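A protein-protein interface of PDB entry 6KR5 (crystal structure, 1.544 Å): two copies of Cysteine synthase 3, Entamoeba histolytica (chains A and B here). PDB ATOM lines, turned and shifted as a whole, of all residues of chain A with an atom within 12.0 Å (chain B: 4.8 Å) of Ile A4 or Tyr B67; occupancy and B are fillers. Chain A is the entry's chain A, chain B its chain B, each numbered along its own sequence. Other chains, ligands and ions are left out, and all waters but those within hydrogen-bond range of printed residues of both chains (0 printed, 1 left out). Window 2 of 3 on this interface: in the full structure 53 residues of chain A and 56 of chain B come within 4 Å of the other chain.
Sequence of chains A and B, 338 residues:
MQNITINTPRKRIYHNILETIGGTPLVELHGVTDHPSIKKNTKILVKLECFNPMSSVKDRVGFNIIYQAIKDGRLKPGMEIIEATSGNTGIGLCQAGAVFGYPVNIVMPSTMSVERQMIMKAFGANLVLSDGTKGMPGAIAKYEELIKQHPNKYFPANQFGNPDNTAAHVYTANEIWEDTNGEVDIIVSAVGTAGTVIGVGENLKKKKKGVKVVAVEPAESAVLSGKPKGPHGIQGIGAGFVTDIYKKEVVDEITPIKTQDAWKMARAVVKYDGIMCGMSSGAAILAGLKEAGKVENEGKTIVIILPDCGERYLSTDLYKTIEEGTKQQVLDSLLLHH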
ATOM      1  N   ASN A   3      29.023  19.232  26.940  1.00  0.00           N
ATOM      2  CA  ASN A   3      29.519  17.967  27.475  1.00  0.00           C
ATOM      3  C   ASN A   3      29.108  16.808  26.575  1.00  0.00           C
ATOM      4  O   ASN A   3      28.268  15.987  26.951  1.00  0.00           O
ATOM      5  CB  ASN A   3      29.009  17.751  28.894  1.00  0.00           C
ATOM      6  N   ILE A   4      29.700  16.742  25.386  1.00  0.00           N
ATOM      7  CA  ILE A   4      29.330  15.742  24.391  1.00  0.00           C
ATOM      8  C   ILE A   4      30.166  14.490  24.607  1.00  0.00           C
ATOM      9  O   ILE A   4      31.401  14.540  24.577  1.00  0.00           O
ATOM     10  CB  ILE A   4      29.511  16.279  22.965  1.00  0.00           C
ATOM     11  CG1 ILE A   4      28.603  17.483  22.738  1.00  0.00           C
ATOM     12  CG2 ILE A   4      29.209  15.190  21.943  1.00  0.00           C
ATOM     13  CD1 ILE A   4      28.683  18.023  21.339  1.00  0.00           C
ATOM     14  N   THR A   5      29.491  13.367  24.809  1.00  0.00           N
ATOM     15  CA  THR A   5      30.125  12.065  24.964  1.00  0.00           C
ATOM     16  C   THR A   5      29.865  11.288  23.683  1.00  0.00           C
ATOM     17  O   THR A   5      28.722  10.917  23.407  1.00  0.00           O
ATOM     18  CB  THR A   5      29.560  11.329  26.177  1.00  0.00           C
ATOM     19  OG1 THR A   5      29.875  12.058  27.372  1.00  0.00           O
ATOM     20  CG2 THR A   5      30.145   9.925  26.281  1.00  0.00           C
ATOM     21  N   ILE A   6      30.936  11.031  22.936  1.00  0.00           N
ATOM     22  CA  ILE A   6      30.776  10.265  21.674  1.00  0.00           C
ATOM     23  C   ILE A   6      30.797   8.766  21.968  1.00  0.00           C
ATOM     24  O   ILE A   6      30.823   8.332  23.120  1.00  0.00           O
ATOM     25  CB  ILE A   6      31.709  10.694  20.521  1.00  0.00           C
ATOM     26  CG1 ILE A   6      33.181  10.443  20.811  1.00  0.00           C
ATOM     27  CG2 ILE A   6      31.477  12.142  20.169  1.00  0.00           C
ATOM     28  CD1 ILE A   6      34.062  10.644  19.613  1.00  0.00           C
ATOM     29  N   ASN A   7      30.820   7.973  20.921  1.00  0.00           N
ATOM     30  CA  ASN A   7      30.694   6.529  21.168  1.00  0.00           C
ATOM     31  C   ASN A   7      31.900   5.974  21.920  1.00  0.00           C
ATOM     32  O   ASN A   7      33.005   6.467  21.812  1.00  0.00           O
ATOM     33  CB  ASN A   7      30.342   5.785  19.893  1.00  0.00           C
ATOM     34  CG  ASN A   7      29.181   4.850  20.077  1.00  0.00           C
ATOM     35  OD1 ASN A   7      28.912   4.420  21.180  1.00  0.00           O
ATOM     36  ND2 ASN A   7      28.464   4.591  19.003  1.00  0.00           N
ATOM     37  N   THR A   8      31.611   4.942  22.682  1.00  0.00           N
ATOM     38  CA  THR A   8      32.651   4.235  23.442  1.00  0.00           C
ATOM     39  C   THR A   8      32.988   3.013  22.624  1.00  0.00           C
ATOM     40  O   THR A   8      32.264   2.598  21.737  1.00  0.00           O
ATOM     41  CB  THR A   8      32.076   3.715  24.755  1.00  0.00           C
ATOM     42  OG1 THR A   8      30.911   2.994  24.385  1.00  0.00           O
ATOM     43  CG2 THR A   8      31.696   4.848  25.668  1.00  0.00           C
ATOM     44  N   VAL A  27      18.284   7.229  19.598  1.00  0.00           N
ATOM     45  CA  VAL A  27      18.748   8.618  19.630  1.00  0.00           C
ATOM     46  C   VAL A  27      17.574   9.560  19.877  1.00  0.00           C
ATOM     47  O   VAL A  27      16.502   9.399  19.282  1.00  0.00           O
ATOM     48  CB  VAL A  27      19.468   8.993  18.315  1.00  0.00           C
ATOM     49  CG1 VAL A  27      20.027  10.446  18.364  1.00  0.00           C
ATOM     50  CG2 VAL A  27      20.578   7.982  18.013  1.00  0.00           C
ATOM     51  N   GLU A  28      17.785  10.560  20.742  1.00  0.00           N
ATOM     52  CA  GLU A  28      16.775  11.593  20.955  1.00  0.00           C
ATOM     53  C   GLU A  28      16.634  12.496  19.734  1.00  0.00           C
ATOM     54  O   GLU A  28      17.629  12.980  19.184  1.00  0.00           O
ATOM     55  CB  GLU A  28      17.137  12.472  22.158  1.00  0.00           C
ATOM     56  CG  GLU A  28      17.294  11.733  23.483  1.00  0.00           C
ATOM     57  CD  GLU A  28      17.805  12.624  24.618  1.00  0.00           C
ATOM     58  OE1 GLU A  28      18.447  13.661  24.348  1.00  0.00           O
ATOM     59  OE2 GLU A  28      17.576  12.265  25.792  1.00  0.00           O
ATOM     60  N   HIS A  30      15.412  16.285  18.649  1.00  0.00           N
ATOM     61  CA  HIS A  30      15.281  17.596  19.287  1.00  0.00           C
ATOM     62  C   HIS A  30      14.862  18.668  18.296  1.00  0.00           C
ATOM     63  O   HIS A  30      14.057  19.545  18.623  1.00  0.00           O
ATOM     64  CB  HIS A  30      16.589  18.030  19.938  1.00  0.00           C
ATOM     65  CG  HIS A  30      17.060  17.116  21.020  1.00  0.00           C
ATOM     66  ND1 HIS A  30      16.438  17.026  22.247  1.00  0.00           N
ATOM     67  CD2 HIS A  30      18.103  16.254  21.060  1.00  0.00           C
ATOM     68  CE1 HIS A  30      17.069  16.134  22.991  1.00  0.00           C
ATOM     69  NE2 HIS A  30      18.087  15.657  22.297  1.00  0.00           N
ATOM     70  N   ASP A 273      17.891  17.773  12.630  1.00  0.00           N
ATOM     71  CA  ASP A 273      18.493  16.845  13.574  1.00  0.00           C
ATOM     72  C   ASP A 273      19.748  16.186  13.034  1.00  0.00           C
ATOM     73  O   ASP A 273      20.388  15.430  13.769  1.00  0.00           O
ATOM     74  CB  ASP A 273      17.482  15.764  13.990  1.00  0.00           C
ATOM     75  CG  ASP A 273      16.487  16.288  14.995  1.00  0.00           C
ATOM     76  OD1 ASP A 273      16.803  16.299  16.205  1.00  0.00           O
ATOM     77  OD2 ASP A 273      15.403  16.722  14.565  1.00  0.00           O
ATOM     78  N   LEU B  18      25.570  13.109  16.906  1.00  0.00           N
ATOM     79  CA  LEU B  18      27.017  13.216  17.055  1.00  0.00           C
ATOM     80  C   LEU B  18      27.543  12.243  18.100  1.00  0.00           C
ATOM     81  O   LEU B  18      28.691  11.790  18.006  1.00  0.00           O
ATOM     82  CB  LEU B  18      27.412  14.645  17.419  1.00  0.00           C
ATOM     83  CG  LEU B  18      26.919  15.696  16.435  1.00  0.00           C
ATOM     84  CD1 LEU B  18      27.523  17.042  16.807  1.00  0.00           C
ATOM     85  CD2 LEU B  18      27.320  15.333  15.013  1.00  0.00           C
ATOM     86  N   GLU B  19      26.724  11.906  19.095  1.00  0.00           N
ATOM     87  CA  GLU B  19      27.160  10.985  20.137  1.00  0.00           C
ATOM     88  C   GLU B  19      27.284   9.551  19.646  1.00  0.00           C
ATOM     89  O   GLU B  19      27.829   8.718  20.376  1.00  0.00           O
ATOM     90  CB  GLU B  19      26.205  11.040  21.328  1.00  0.00           C
ATOM     91  CG  GLU B  19      26.231  12.402  22.009  1.00  0.00           C
ATOM     92  CD  GLU B  19      25.639  12.398  23.407  1.00  0.00           C
ATOM     93  OE1 GLU B  19      24.841  11.502  23.737  1.00  0.00           O
ATOM     94  OE2 GLU B  19      25.989  13.316  24.182  1.00  0.00           O
ATOM     95  N   PHE B  63      33.493  16.336  13.021  1.00  0.00           N
ATOM     96  CA  PHE B  63      33.042  16.574  14.384  1.00  0.00           C
ATOM     97  C   PHE B  63      34.130  17.233  15.216  1.00  0.00           C
ATOM     98  O   PHE B  63      33.890  18.258  15.860  1.00  0.00           O
ATOM     99  CB  PHE B  63      32.614  15.267  15.045  1.00  0.00           C
ATOM    100  CG  PHE B  63      32.387  15.412  16.518  1.00  0.00           C
ATOM    101  CD1 PHE B  63      31.221  16.001  16.985  1.00  0.00           C
ATOM    102  CD2 PHE B  63      33.344  15.011  17.431  1.00  0.00           C
ATOM    103  CE1 PHE B  63      31.000  16.154  18.342  1.00  0.00           C
ATOM    104  CE2 PHE B  63      33.130  15.174  18.790  1.00  0.00           C
ATOM    105  CZ  PHE B  63      31.966  15.748  19.241  1.00  0.00           C
ATOM    106  N   ASN B  64      35.332  16.649  15.247  1.00  0.00           N
ATOM    107  CA  ASN B  64      36.331  17.201  16.160  1.00  0.00           C
ATOM    108  C   ASN B  64      36.871  18.548  15.695  1.00  0.00           C
ATOM    109  O   ASN B  64      37.199  19.395  16.536  1.00  0.00           O
ATOM    110  CB  ASN B  64      37.494  16.236  16.382  1.00  0.00           C
ATOM    111  CG  ASN B  64      38.215  16.543  17.674  1.00  0.00           C
ATOM    112  OD1 ASN B  64      37.591  16.541  18.745  1.00  0.00           O
ATOM    113  ND2 ASN B  64      39.505  16.871  17.588  1.00  0.00           N
ATOM    114  N   ILE B  65      37.002  18.770  14.384  1.00  0.00           N
ATOM    115  CA  ILE B  65      37.434  20.087  13.905  1.00  0.00           C
ATOM    116  C   ILE B  65      36.475  21.166  14.397  1.00  0.00           C
ATOM    117  O   ILE B  65      36.895  22.204  14.919  1.00  0.00           O
ATOM    118  CB  ILE B  65      37.551  20.079  12.369  1.00  0.00           C
ATOM    119  CG1 ILE B  65      38.861  19.392  11.956  1.00  0.00           C
ATOM    120  CG2 ILE B  65      37.462  21.491  11.804  1.00  0.00           C
ATOM    121  CD1 ILE B  65      38.976  19.139  10.491  1.00  0.00           C
ATOM    122  N   ILE B  66      35.174  20.916  14.287  1.00  0.00           N
ATOM    123  CA  ILE B  66      34.198  21.924  14.683  1.00  0.00           C
ATOM    124  C   ILE B  66      34.074  22.003  16.201  1.00  0.00           C
ATOM    125  O   ILE B  66      34.042  23.101  16.772  1.00  0.00           O
ATOM    126  CB  ILE B  66      32.853  21.624  14.005  1.00  0.00           C
ATOM    127  CG1 ILE B  66      32.994  21.831  12.498  1.00  0.00           C
ATOM    128  CG2 ILE B  66      31.769  22.531  14.553  1.00  0.00           C
ATOM    129  CD1 ILE B  66      31.848  21.239  11.696  1.00  0.00           C
ATOM    130  N   TYR B  67      34.023  20.851  16.875  1.00  0.00           N
ATOM    131  CA  TYR B  67      33.872  20.827  18.328  1.00  0.00           C
ATOM    132  C   TYR B  67      35.019  21.556  19.005  1.00  0.00           C
ATOM    133  O   TYR B  67      34.806  22.395  19.888  1.00  0.00           O
ATOM    134  CB  TYR B  67      33.806  19.382  18.808  1.00  0.00           C
ATOM    135  CG  TYR B  67      33.424  19.184  20.255  1.00  0.00           C
ATOM    136  CD1 TYR B  67      32.489  20.005  20.870  1.00  0.00           C
ATOM    137  CD2 TYR B  67      33.969  18.145  20.989  1.00  0.00           C
ATOM    138  CE1 TYR B  67      32.127  19.803  22.189  1.00  0.00           C
ATOM    139  CE2 TYR B  67      33.618  17.937  22.307  1.00  0.00           C
ATOM    140  CZ  TYR B  67      32.698  18.767  22.904  1.00  0.00           C
ATOM    141  OH  TYR B  67      32.344  18.556  24.218  1.00  0.00           O
ATOM    142  N   GLN B  68      36.250  21.241  18.608  1.00  0.00           N
ATOM    143  CA  GLN B  68      37.385  21.879  19.264  1.00  0.00           C
ATOM    144  C   GLN B  68      37.419  23.370  18.969  1.00  0.00           C
ATOM    145  O   GLN B  68      37.766  24.176  19.846  1.00  0.00           O
ATOM    146  CB  GLN B  68      38.691  21.222  18.831  1.00  0.00           C
ATOM    147  CG  GLN B  68      39.865  21.626  19.733  1.00  0.00           C
ATOM    148  CD  GLN B  68      39.708  21.090  21.147  1.00  0.00           C
ATOM    149  OE1 GLN B  68      39.455  19.907  21.345  1.00  0.00           O
ATOM    150  NE2 GLN B  68      39.850  21.965  22.138  1.00  0.00           N
ATOM    151  N   ALA B  69      37.055  23.763  17.743  1.00  0.00           N
ATOM    152  CA  ALA B  69      37.056  25.185  17.408  1.00  0.00           C
ATOM    153  C   ALA B  69      36.041  25.941  18.250  1.00  0.00           C
ATOM    154  O   ALA B  69      36.307  27.067  18.689  1.00  0.00           O
ATOM    155  CB  ALA B  69      36.779  25.395  15.919  1.00  0.00           C
ATOM    156  N   ILE B  70      34.875  25.340  18.499  1.00  0.00           N
ATOM    157  CA  ILE B  70      33.893  25.982  19.368  1.00  0.00           C
ATOM    158  C   ILE B  70      34.437  26.101  20.785  1.00  0.00           C
ATOM    159  O   ILE B  70      34.362  27.166  21.409  1.00  0.00           O
ATOM    160  CB  ILE B  70      32.561  25.217  19.343  1.00  0.00           C
ATOM    161  CG1 ILE B  70      31.910  25.359  17.968  1.00  0.00           C
ATOM    162  CG2 ILE B  70      31.638  25.755  20.415  1.00  0.00           C
ATOM    163  CD1 ILE B  70      30.745  24.414  17.727  1.00  0.00           C
ATOM    164  N   LYS B  71      35.014  25.015  21.303  1.00  0.00           N
ATOM    165  CA  LYS B  71      35.529  25.028  22.670  1.00  0.00           C
ATOM    166  C   LYS B  71      36.646  26.052  22.837  1.00  0.00           C
ATOM    167  O   LYS B  71      36.744  26.705  23.885  1.00  0.00           O
ATOM    168  CB  LYS B  71      36.019  23.632  23.060  1.00  0.00           C
ATOM    169  CG  LYS B  71      34.890  22.621  23.253  1.00  0.00           C
ATOM    170  CD  LYS B  71      35.364  21.359  23.966  1.00  0.00           C
ATOM    171  CE  LYS B  71      36.329  20.561  23.107  1.00  0.00           C
ATOM    172  NZ  LYS B  71      36.579  19.209  23.679  1.00  0.00           N
ATOM    173  N   PHE B 100      25.537  21.321  15.596  1.00  0.00           N
ATOM    174  CA  PHE B 100      26.052  22.427  16.400  1.00  0.00           C
ATOM    175  C   PHE B 100      25.402  23.754  16.045  1.00  0.00           C
ATOM    176  O   PHE B 100      25.556  24.721  16.801  1.00  0.00           O
ATOM    177  CB  PHE B 100      27.568  22.561  16.236  1.00  0.00           C
ATOM    178  CG  PHE B 100      28.358  21.553  17.014  1.00  0.00           C
ATOM    179  CD1 PHE B 100      28.315  21.539  18.399  1.00  0.00           C
ATOM    180  CD2 PHE B 100      29.172  20.638  16.366  1.00  0.00           C
ATOM    181  CE1 PHE B 100      29.051  20.605  19.128  1.00  0.00           C
ATOM    182  CE2 PHE B 100      29.917  19.702  17.088  1.00  0.00           C
ATOM    183  CZ  PHE B 100      29.858  19.687  18.466  1.00  0.00           C
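The side-chain hydroxyl (OH) of Tyr B67 is in hydrogen-bond range of the backbone NH (N) of Ile A4 (3.4 Å).
O of Glu B19 lies within hydrogen-bond range of N of Asn A7 (3.1 Å).
Among the printed residues, pairs that only touch across the chains: Thr A5 with Glu B19 (3.2 Å), Ile A6 with Glu B19 (3.4 Å), Ile A4 with Phe B100 (3.4 Å), Ile A6 with Leu B18 (3.5 Å), Ile A6 with Phe B63 (3.7 Å) and Ile A4 with Phe B63 (3.9 Å).
Ile A4 touches just these residues of chain B: Phe B63 (3.9 Å), Tyr B67 (3.4 Å) and Phe B100 (3.4 Å).
Of the printed residues of chain A, Tyr B67 touches Ile A4.
Of chain A, only Ile A6 comes within 4 Å of Leu B18.
Glu B19 touches just these residues of chain A: Thr A5, Ile A6 and Asn A7.
No residue of chain A comes within 4 Å of Asn B64.
No residue of chain A comes within 4 Å of Ile B66.
No residue of chain A comes within 4 Å of Ala B69.
No residue of chain A comes within 4 Å of Ile B70.
Printed residues of chain A within 4 Å of Phe B100: Ile A4 (3.4 Å).
Of the printed residues of chain B, Ile A6 touches Leu B18, Glu B19 and Phe B63.
Printed residues of chain B within 4 Å of Asn A7: Glu B19.
The nearest residue of chain B that does not touch Ile A4 is Glu B19 (4.1 Å).
The nearest residue of chain A that does not touch Tyr B67 is Asn A3 (4.3 Å).
Hydrophobic or aromatic side chains of chain B that line the printed part of chain A: Phe B63, Tyr B67 and Phe B100.
Of the 10 printed residues of chain A, 4 touch a printed residue of chain B.
Hydrophobic or aromatic side chains of chain A that line the printed part of chain B: Ile A4 and Ile A6.
Along chain A the printed residues that touch a printed residue of chain B span positions 4 to 7.
Among the printed residues, 8 pairs touch across the chains.
Among the printed residues, no Asp or Glu carboxylate lies within 4 Å of a Lys or Arg side-chain nitrogen of the other chain.
No position is printed for both chains.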
